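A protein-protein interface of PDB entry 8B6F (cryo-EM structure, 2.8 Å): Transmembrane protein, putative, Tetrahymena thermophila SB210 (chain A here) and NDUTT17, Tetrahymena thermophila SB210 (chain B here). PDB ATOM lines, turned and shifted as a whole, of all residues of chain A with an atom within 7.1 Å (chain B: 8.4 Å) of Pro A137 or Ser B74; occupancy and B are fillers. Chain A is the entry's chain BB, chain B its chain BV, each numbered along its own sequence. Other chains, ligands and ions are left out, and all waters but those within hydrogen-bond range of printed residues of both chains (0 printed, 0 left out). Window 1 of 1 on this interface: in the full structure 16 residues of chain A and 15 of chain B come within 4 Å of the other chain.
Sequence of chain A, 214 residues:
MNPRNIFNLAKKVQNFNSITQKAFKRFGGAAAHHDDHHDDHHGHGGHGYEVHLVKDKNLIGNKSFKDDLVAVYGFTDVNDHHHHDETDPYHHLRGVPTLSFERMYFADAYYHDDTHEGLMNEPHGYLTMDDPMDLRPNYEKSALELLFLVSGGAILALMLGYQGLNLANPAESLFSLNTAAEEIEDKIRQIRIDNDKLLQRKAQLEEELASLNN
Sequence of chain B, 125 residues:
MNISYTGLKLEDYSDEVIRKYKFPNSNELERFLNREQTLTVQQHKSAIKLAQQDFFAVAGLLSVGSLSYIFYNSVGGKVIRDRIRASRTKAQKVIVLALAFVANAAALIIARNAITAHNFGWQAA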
ATOM      1  N   ASP A 134      31.015  24.657   0.869  1.00  0.00           N
ATOM      2  CA  ASP A 134      30.499  24.077   2.100  1.00  0.00           C
ATOM      3  C   ASP A 134      31.098  22.692   2.273  1.00  0.00           C
ATOM      4  O   ASP A 134      31.108  21.893   1.330  1.00  0.00           O
ATOM      5  CB  ASP A 134      28.971  23.996   2.065  1.00  0.00           C
ATOM      6  CG  ASP A 134      28.373  23.679   3.418  1.00  0.00           C
ATOM      7  OD1 ASP A 134      29.133  23.622   4.407  1.00  0.00           O
ATOM      8  OD2 ASP A 134      27.143  23.488   3.494  1.00  0.00           O
ATOM      9  N   LEU A 135      31.597  22.408   3.473  1.00  0.00           N
ATOM     10  CA  LEU A 135      32.234  21.133   3.761  1.00  0.00           C
ATOM     11  C   LEU A 135      31.263  20.086   4.288  1.00  0.00           C
ATOM     12  O   LEU A 135      31.678  18.951   4.539  1.00  0.00           O
ATOM     13  CB  LEU A 135      33.376  21.328   4.766  1.00  0.00           C
ATOM     14  CG  LEU A 135      34.516  22.290   4.397  1.00  0.00           C
ATOM     15  CD1 LEU A 135      35.004  22.057   2.972  1.00  0.00           C
ATOM     16  CD2 LEU A 135      34.126  23.750   4.600  1.00  0.00           C
ATOM     17  N   ARG A 136      29.992  20.433   4.463  1.00  0.00           N
ATOM     18  CA  ARG A 136      29.014  19.475   4.958  1.00  0.00           C
ATOM     19  C   ARG A 136      28.615  18.507   3.846  1.00  0.00           C
ATOM     20  O   ARG A 136      28.357  18.933   2.719  1.00  0.00           O
ATOM     21  CB  ARG A 136      27.774  20.192   5.484  1.00  0.00           C
ATOM     22  CG  ARG A 136      28.023  20.999   6.739  1.00  0.00           C
ATOM     23  CD  ARG A 136      26.733  21.539   7.326  1.00  0.00           C
ATOM     24  NE  ARG A 136      26.133  22.562   6.480  1.00  0.00           N
ATOM     25  CZ  ARG A 136      25.032  23.236   6.786  1.00  0.00           C
ATOM     26  NH1 ARG A 136      24.378  23.017   7.913  1.00  0.00           N
ATOM     27  NH2 ARG A 136      24.580  24.157   5.941  1.00  0.00           N
ATOM     28  N   PRO A 137      28.547  17.201   4.127  1.00  0.00           N
ATOM     29  CA  PRO A 137      27.999  16.265   3.130  1.00  0.00           C
ATOM     30  C   PRO A 137      26.474  16.296   3.095  1.00  0.00           C
ATOM     31  O   PRO A 137      25.791  15.291   3.309  1.00  0.00           O
ATOM     32  CB  PRO A 137      28.559  14.918   3.607  1.00  0.00           C
ATOM     33  CG  PRO A 137      28.655  15.064   5.075  1.00  0.00           C
ATOM     34  CD  PRO A 137      29.013  16.501   5.338  1.00  0.00           C
ATOM     35  N   ASN A 138      25.932  17.479   2.826  1.00  0.00           N
ATOM     36  CA  ASN A 138      24.492  17.684   2.835  1.00  0.00           C
ATOM     37  C   ASN A 138      23.845  17.023   1.623  1.00  0.00           C
ATOM     38  O   ASN A 138      24.390  17.057   0.517  1.00  0.00           O
ATOM     39  CB  ASN A 138      24.186  19.180   2.852  1.00  0.00           C
ATOM     40  CG  ASN A 138      22.716  19.470   3.004  1.00  0.00           C
ATOM     41  OD1 ASN A 138      21.936  18.598   3.377  1.00  0.00           O
ATOM     42  ND2 ASN A 138      22.328  20.704   2.721  1.00  0.00           N
ATOM     43  N   TYR A 139      22.671  16.415   1.832  1.00  0.00           N
ATOM     44  CA  TYR A 139      22.009  15.649   0.781  1.00  0.00           C
ATOM     45  C   TYR A 139      20.560  16.057   0.549  1.00  0.00           C
ATOM     46  O   TYR A 139      19.845  15.351  -0.171  1.00  0.00           O
ATOM     47  CB  TYR A 139      22.059  14.147   1.090  1.00  0.00           C
ATOM     48  CG  TYR A 139      21.404  13.753   2.391  1.00  0.00           C
ATOM     49  CD1 TYR A 139      20.040  13.514   2.468  1.00  0.00           C
ATOM     50  CD2 TYR A 139      22.161  13.604   3.542  1.00  0.00           C
ATOM     51  CE1 TYR A 139      19.450  13.147   3.660  1.00  0.00           C
ATOM     52  CE2 TYR A 139      21.580  13.239   4.735  1.00  0.00           C
ATOM     53  CZ  TYR A 139      20.226  13.012   4.788  1.00  0.00           C
ATOM     54  OH  TYR A 139      19.651  12.648   5.979  1.00  0.00           O
ATOM     55  N   GLU A 140      20.099  17.163   1.132  1.00  0.00           N
ATOM     56  CA  GLU A 140      18.727  17.585   0.878  1.00  0.00           C
ATOM     57  C   GLU A 140      18.536  17.980  -0.583  1.00  0.00           C
ATOM     58  O   GLU A 140      17.536  17.609  -1.206  1.00  0.00           O
ATOM     59  CB  GLU A 140      18.349  18.739   1.804  1.00  0.00           C
ATOM     60  CG  GLU A 140      19.208  19.975   1.637  1.00  0.00           C
ATOM     61  CD  GLU A 140      18.945  21.013   2.707  1.00  0.00           C
ATOM     62  OE1 GLU A 140      18.309  20.668   3.723  1.00  0.00           O
ATOM     63  OE2 GLU A 140      19.367  22.173   2.528  1.00  0.00           O
ATOM     64  N   SER A 142      20.308  16.951  -3.179  1.00  0.00           N
ATOM     65  CA  SER A 142      20.376  15.737  -3.983  1.00  0.00           C
ATOM     66  C   SER A 142      19.086  14.937  -3.876  1.00  0.00           C
ATOM     67  O   SER A 142      18.616  14.367  -4.867  1.00  0.00           O
ATOM     68  CB  SER A 142      21.574  14.890  -3.557  1.00  0.00           C
ATOM     69  OG  SER A 142      21.445  14.465  -2.212  1.00  0.00           O
ATOM     70  N   LEU B  67      20.824   5.647  -3.644  1.00  0.00           N
ATOM     71  CA  LEU B  67      21.950   5.783  -2.726  1.00  0.00           C
ATOM     72  C   LEU B  67      23.209   6.233  -3.454  1.00  0.00           C
ATOM     73  O   LEU B  67      23.956   7.078  -2.950  1.00  0.00           O
ATOM     74  CB  LEU B  67      22.186   4.464  -1.992  1.00  0.00           C
ATOM     75  CG  LEU B  67      21.066   4.038  -1.035  1.00  0.00           C
ATOM     76  CD1 LEU B  67      21.356   2.675  -0.431  1.00  0.00           C
ATOM     77  CD2 LEU B  67      20.861   5.068   0.065  1.00  0.00           C
ATOM     78  N   SER B  68      23.462   5.685  -4.642  1.00  0.00           N
ATOM     79  CA  SER B  68      24.646   6.087  -5.393  1.00  0.00           C
ATOM     80  C   SER B  68      24.575   7.561  -5.764  1.00  0.00           C
ATOM     81  O   SER B  68      25.557   8.298  -5.623  1.00  0.00           O
ATOM     82  CB  SER B  68      24.794   5.222  -6.645  1.00  0.00           C
ATOM     83  OG  SER B  68      23.674   5.364  -7.497  1.00  0.00           O
ATOM     84  N   TYR B  69      23.417   8.009  -6.247  1.00  0.00           N
ATOM     85  CA  TYR B  69      23.262   9.414  -6.602  1.00  0.00           C
ATOM     86  C   TYR B  69      23.482  10.303  -5.385  1.00  0.00           C
ATOM     87  O   TYR B  69      24.175  11.324  -5.462  1.00  0.00           O
ATOM     88  CB  TYR B  69      21.874   9.645  -7.202  1.00  0.00           C
ATOM     89  CG  TYR B  69      21.619  11.064  -7.655  1.00  0.00           C
ATOM     90  CD1 TYR B  69      21.103  12.011  -6.783  1.00  0.00           C
ATOM     91  CD2 TYR B  69      21.880  11.451  -8.963  1.00  0.00           C
ATOM     92  CE1 TYR B  69      20.863  13.307  -7.196  1.00  0.00           C
ATOM     93  CE2 TYR B  69      21.644  12.744  -9.386  1.00  0.00           C
ATOM     94  CZ  TYR B  69      21.134  13.666  -8.497  1.00  0.00           C
ATOM     95  OH  TYR B  69      20.896  14.956  -8.913  1.00  0.00           O
ATOM     96  N   ILE B  70      22.886   9.932  -4.250  1.00  0.00           N
ATOM     97  CA  ILE B  70      23.014  10.741  -3.041  1.00  0.00           C
ATOM     98  C   ILE B  70      24.473  10.841  -2.619  1.00  0.00           C
ATOM     99  O   ILE B  70      25.000  11.935  -2.393  1.00  0.00           O
ATOM    100  CB  ILE B  70      22.149  10.153  -1.912  1.00  0.00           C
ATOM    101  CG1 ILE B  70      20.674  10.150  -2.311  1.00  0.00           C
ATOM    102  CG2 ILE B  70      22.333  10.935  -0.623  1.00  0.00           C
ATOM    103  CD1 ILE B  70      19.905   9.014  -1.694  1.00  0.00           C
ATOM    104  N   PHE B  71      25.153   9.697  -2.521  1.00  0.00           N
ATOM    105  CA  PHE B  71      26.516   9.695  -2.003  1.00  0.00           C
ATOM    106  C   PHE B  71      27.497  10.353  -2.961  1.00  0.00           C
ATOM    107  O   PHE B  71      28.496  10.931  -2.518  1.00  0.00           O
ATOM    108  CB  PHE B  71      26.950   8.265  -1.685  1.00  0.00           C
ATOM    109  CG  PHE B  71      26.495   7.785  -0.337  1.00  0.00           C
ATOM    110  CD1 PHE B  71      25.180   7.408  -0.125  1.00  0.00           C
ATOM    111  CD2 PHE B  71      27.384   7.718   0.721  1.00  0.00           C
ATOM    112  CE1 PHE B  71      24.761   6.972   1.118  1.00  0.00           C
ATOM    113  CE2 PHE B  71      26.972   7.285   1.965  1.00  0.00           C
ATOM    114  CZ  PHE B  71      25.659   6.911   2.164  1.00  0.00           C
ATOM    115  N   TYR B  72      27.243  10.277  -4.267  1.00  0.00           N
ATOM    116  CA  TYR B  72      28.138  10.909  -5.228  1.00  0.00           C
ATOM    117  C   TYR B  72      27.922  12.412  -5.331  1.00  0.00           C
ATOM    118  O   TYR B  72      28.883  13.152  -5.563  1.00  0.00           O
ATOM    119  CB  TYR B  72      27.964  10.273  -6.606  1.00  0.00           C
ATOM    120  CG  TYR B  72      28.347   8.811  -6.678  1.00  0.00           C
ATOM    121  CD1 TYR B  72      29.289   8.271  -5.811  1.00  0.00           C
ATOM    122  CD2 TYR B  72      27.768   7.971  -7.619  1.00  0.00           C
ATOM    123  CE1 TYR B  72      29.639   6.939  -5.879  1.00  0.00           C
ATOM    124  CE2 TYR B  72      28.111   6.637  -7.694  1.00  0.00           C
ATOM    125  CZ  TYR B  72      29.048   6.127  -6.821  1.00  0.00           C
ATOM    126  OH  TYR B  72      29.394   4.797  -6.893  1.00  0.00           O
ATOM    127  N   ASN B  73      26.685  12.884  -5.168  1.00  0.00           N
ATOM    128  CA  ASN B  73      26.368  14.297  -5.328  1.00  0.00           C
ATOM    129  C   ASN B  73      26.078  14.989  -4.001  1.00  0.00           C
ATOM    130  O   ASN B  73      25.466  16.061  -3.989  1.00  0.00           O
ATOM    131  CB  ASN B  73      25.182  14.464  -6.278  1.00  0.00           C
ATOM    132  CG  ASN B  73      25.492  13.990  -7.683  1.00  0.00           C
ATOM    133  OD1 ASN B  73      25.999  14.750  -8.507  1.00  0.00           O
ATOM    134  ND2 ASN B  73      25.183  12.730  -7.964  1.00  0.00           N
ATOM    135  N   SER B  74      26.501  14.403  -2.887  1.00  0.00           N
ATOM    136  CA  SER B  74      26.310  14.981  -1.560  1.00  0.00           C
ATOM    137  C   SER B  74      27.635  15.096  -0.832  1.00  0.00           C
ATOM    138  O   SER B  74      27.771  14.701   0.328  1.00  0.00           O
ATOM    139  CB  SER B  74      25.358  14.155  -0.710  1.00  0.00           C
ATOM    140  OG  SER B  74      25.184  14.789   0.542  1.00  0.00           O
ATOM    141  N   VAL B  75      28.638  15.648  -1.504  1.00  0.00           N
ATOM    142  CA  VAL B  75      29.962  15.760  -0.908  1.00  0.00           C
ATOM    143  C   VAL B  75      30.243  17.148  -0.337  1.00  0.00           C
ATOM    144  O   VAL B  75      31.143  17.285   0.506  1.00  0.00           O
ATOM    145  CB  VAL B  75      31.049  15.367  -1.928  1.00  0.00           C
ATOM    146  CG1 VAL B  75      32.395  15.280  -1.250  1.00  0.00           C
ATOM    147  CG2 VAL B  75      30.702  14.048  -2.603  1.00  0.00           C
ATOM    148  N   GLY B  76      29.499  18.166  -0.748  1.00  0.00           N
ATOM    149  CA  GLY B  76      29.731  19.509  -0.252  1.00  0.00           C
ATOM    150  C   GLY B  76      29.085  20.528  -1.171  1.00  0.00           C
ATOM    151  O   GLY B  76      28.136  20.223  -1.888  1.00  0.00           O
ATOM    152  N   GLY B  77      29.625  21.740  -1.129  1.00  0.00           N
ATOM    153  CA  GLY B  77      29.134  22.813  -1.964  1.00  0.00           C
ATOM    154  C   GLY B  77      29.485  22.591  -3.421  1.00  0.00           C
ATOM    155  O   GLY B  77      30.149  21.629  -3.805  1.00  0.00           O
ATOM    156  N   ILE B  80      33.294  22.611  -4.082  1.00  0.00           N
ATOM    157  CA  ILE B  80      33.939  21.407  -3.565  1.00  0.00           C
ATOM    158  C   ILE B  80      33.610  20.210  -4.447  1.00  0.00           C
ATOM    159  O   ILE B  80      34.490  19.416  -4.802  1.00  0.00           O
ATOM    160  CB  ILE B  80      33.522  21.164  -2.103  1.00  0.00           C
ATOM    161  CG1 ILE B  80      33.807  22.403  -1.245  1.00  0.00           C
ATOM    162  CG2 ILE B  80      34.237  19.948  -1.534  1.00  0.00           C
ATOM    163  CD1 ILE B  80      35.243  22.886  -1.291  1.00  0.00           C
ATOM    164  N   ARG B  81      32.337  20.062  -4.818  1.00  0.00           N
ATOM    165  CA  ARG B  81      31.938  18.942  -5.665  1.00  0.00           C
ATOM    166  C   ARG B  81      32.616  19.008  -7.024  1.00  0.00           C
ATOM    167  O   ARG B  81      33.075  17.986  -7.548  1.00  0.00           O
ATOM    168  CB  ARG B  81      30.420  18.922  -5.833  1.00  0.00           C
ATOM    169  CG  ARG B  81      29.663  18.570  -4.567  1.00  0.00           C
ATOM    170  CD  ARG B  81      28.167  18.584  -4.806  1.00  0.00           C
ATOM    171  NE  ARG B  81      27.693  19.906  -5.195  1.00  0.00           N
ATOM    172  CZ  ARG B  81      26.432  20.193  -5.488  1.00  0.00           C
ATOM    173  NH1 ARG B  81      25.487  19.269  -5.453  1.00  0.00           N
ATOM    174  NH2 ARG B  81      26.112  21.439  -5.822  1.00  0.00           N
ATOM    175  N   ILE B  84      36.292  18.002  -6.635  1.00  0.00           N
ATOM    176  CA  ILE B  84      36.423  16.568  -6.392  1.00  0.00           C
ATOM    177  C   ILE B  84      36.207  15.790  -7.682  1.00  0.00           C
ATOM    178  O   ILE B  84      36.957  14.858  -7.996  1.00  0.00           O
ATOM    179  CB  ILE B  84      35.453  16.122  -5.283  1.00  0.00           C
ATOM    180  CG1 ILE B  84      35.935  16.672  -3.940  1.00  0.00           C
ATOM    181  CG2 ILE B  84      35.333  14.598  -5.241  1.00  0.00           C
ATOM    182  CD1 ILE B  84      34.992  16.450  -2.806  1.00  0.00           C
ATOM    183  N   ARG B  85      35.180  16.155  -8.448  1.00  0.00           N
ATOM    184  CA  ARG B  85      34.919  15.463  -9.704  1.00  0.00           C
ATOM    185  C   ARG B  85      36.022  15.722 -10.722  1.00  0.00           C
ATOM    186  O   ARG B  85      36.336  14.840 -11.527  1.00  0.00           O
ATOM    187  CB  ARG B  85      33.561  15.884 -10.265  1.00  0.00           C
ATOM    188  CG  ARG B  85      33.138  15.092 -11.492  1.00  0.00           C
ATOM    189  CD  ARG B  85      31.633  15.134 -11.707  1.00  0.00           C
ATOM    190  NE  ARG B  85      30.908  14.496 -10.615  1.00  0.00           N
ATOM    191  CZ  ARG B  85      29.607  14.237 -10.626  1.00  0.00           C
ATOM    192  NH1 ARG B  85      28.850  14.536 -11.670  1.00  0.00           N
ATOM    193  NH2 ARG B  85      29.052  13.662  -9.564  1.00  0.00           N
ATOM    194  N   ARG B  88      38.667  13.521  -9.927  1.00  0.00           N
ATOM    195  CA  ARG B  88      38.208  12.154 -10.109  1.00  0.00           C
ATOM    196  C   ARG B  88      38.767  11.563 -11.398  1.00  0.00           C
ATOM    197  O   ARG B  88      38.865  12.243 -12.422  1.00  0.00           O
ATOM    198  CB  ARG B  88      36.679  12.145 -10.133  1.00  0.00           C
ATOM    199  CG  ARG B  88      36.024  10.791 -10.095  1.00  0.00           C
ATOM    200  CD  ARG B  88      34.573  10.940  -9.676  1.00  0.00           C
ATOM    201  NE  ARG B  88      34.450  11.061  -8.228  1.00  0.00           N
ATOM    202  CZ  ARG B  88      33.364  11.484  -7.596  1.00  0.00           C
ATOM    203  NH1 ARG B  88      32.284  11.867  -8.257  1.00  0.00           N
ATOM    204  NH2 ARG B  88      33.361  11.521  -6.267  1.00  0.00           N
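N of Tyr A139 lies close to OG of Ser B74, at 3.3 Å.
The backbone carbonyl oxygen (O) of Pro A137 is in hydrogen-bond range of the side-chain hydroxyl (OG) of Ser B74, 2.9 Å away.
O of Asn A138 lies within hydrogen-bond range of OG of Ser B74.
N of Gly B77 lies within hydrogen-bond range of O of Asp A134, at 2.9 Å.
The side-chain amide nitrogen (ND2) of Asn B73 lies within hydrogen-bond range of the backbone carbonyl oxygen (O) of Tyr B69 (3.0 Å).
NE of Arg B81 lies close to O of Gly B76, at 3.4 Å.
The side-chain carboxylate (OD2) of Asp A134 is in salt-bridge range of the guanidinium group (NE) of Arg A136, at 3.3 Å.
The side-chain amide oxygen (OD1) of Asn A138 sits at hydrogen-bond distance from the backbone NH (N) of Glu A140 (3.2 Å).
NE of Arg B81 sits close to O of Gly B77.
O of Tyr A139 is in hydrogen-bond range of OG of Ser A142 (2.7 Å).
Asp A134 touches Gly B76.
Asp A134 touches Ile B80.
Arg A136 touches Val B75 (O to O, 3.9 Å).
O of Arg A136 touches CA of Gly B76 (3.3 Å).
Ile B70 touches Tyr A139.
O of Ser A142 touches CE1 of Tyr B69, 3.4 Å away.
Ser A142 touches Ile B70.
Of chain B, only Ser B74 comes within 4 Å of Pro A137.
Glu A140 touches none of the printed residues of chain B.
Of the printed residues of chain B, Ser A142 touches Tyr B69 (3.4 Å) and Ile B70 (3.97 Å).
Printed residues of chain A within 4 Å of Tyr B69: Ser A142 (3.4 Å).
Phe B71 touches none of the printed residues of chain A.
Ser B74 touches three residues of chain A.
Of the printed residues of chain A, Val B75 touches Arg A136 (3.9 Å).
Among the printed residues, 11 pairs touch across the chains.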
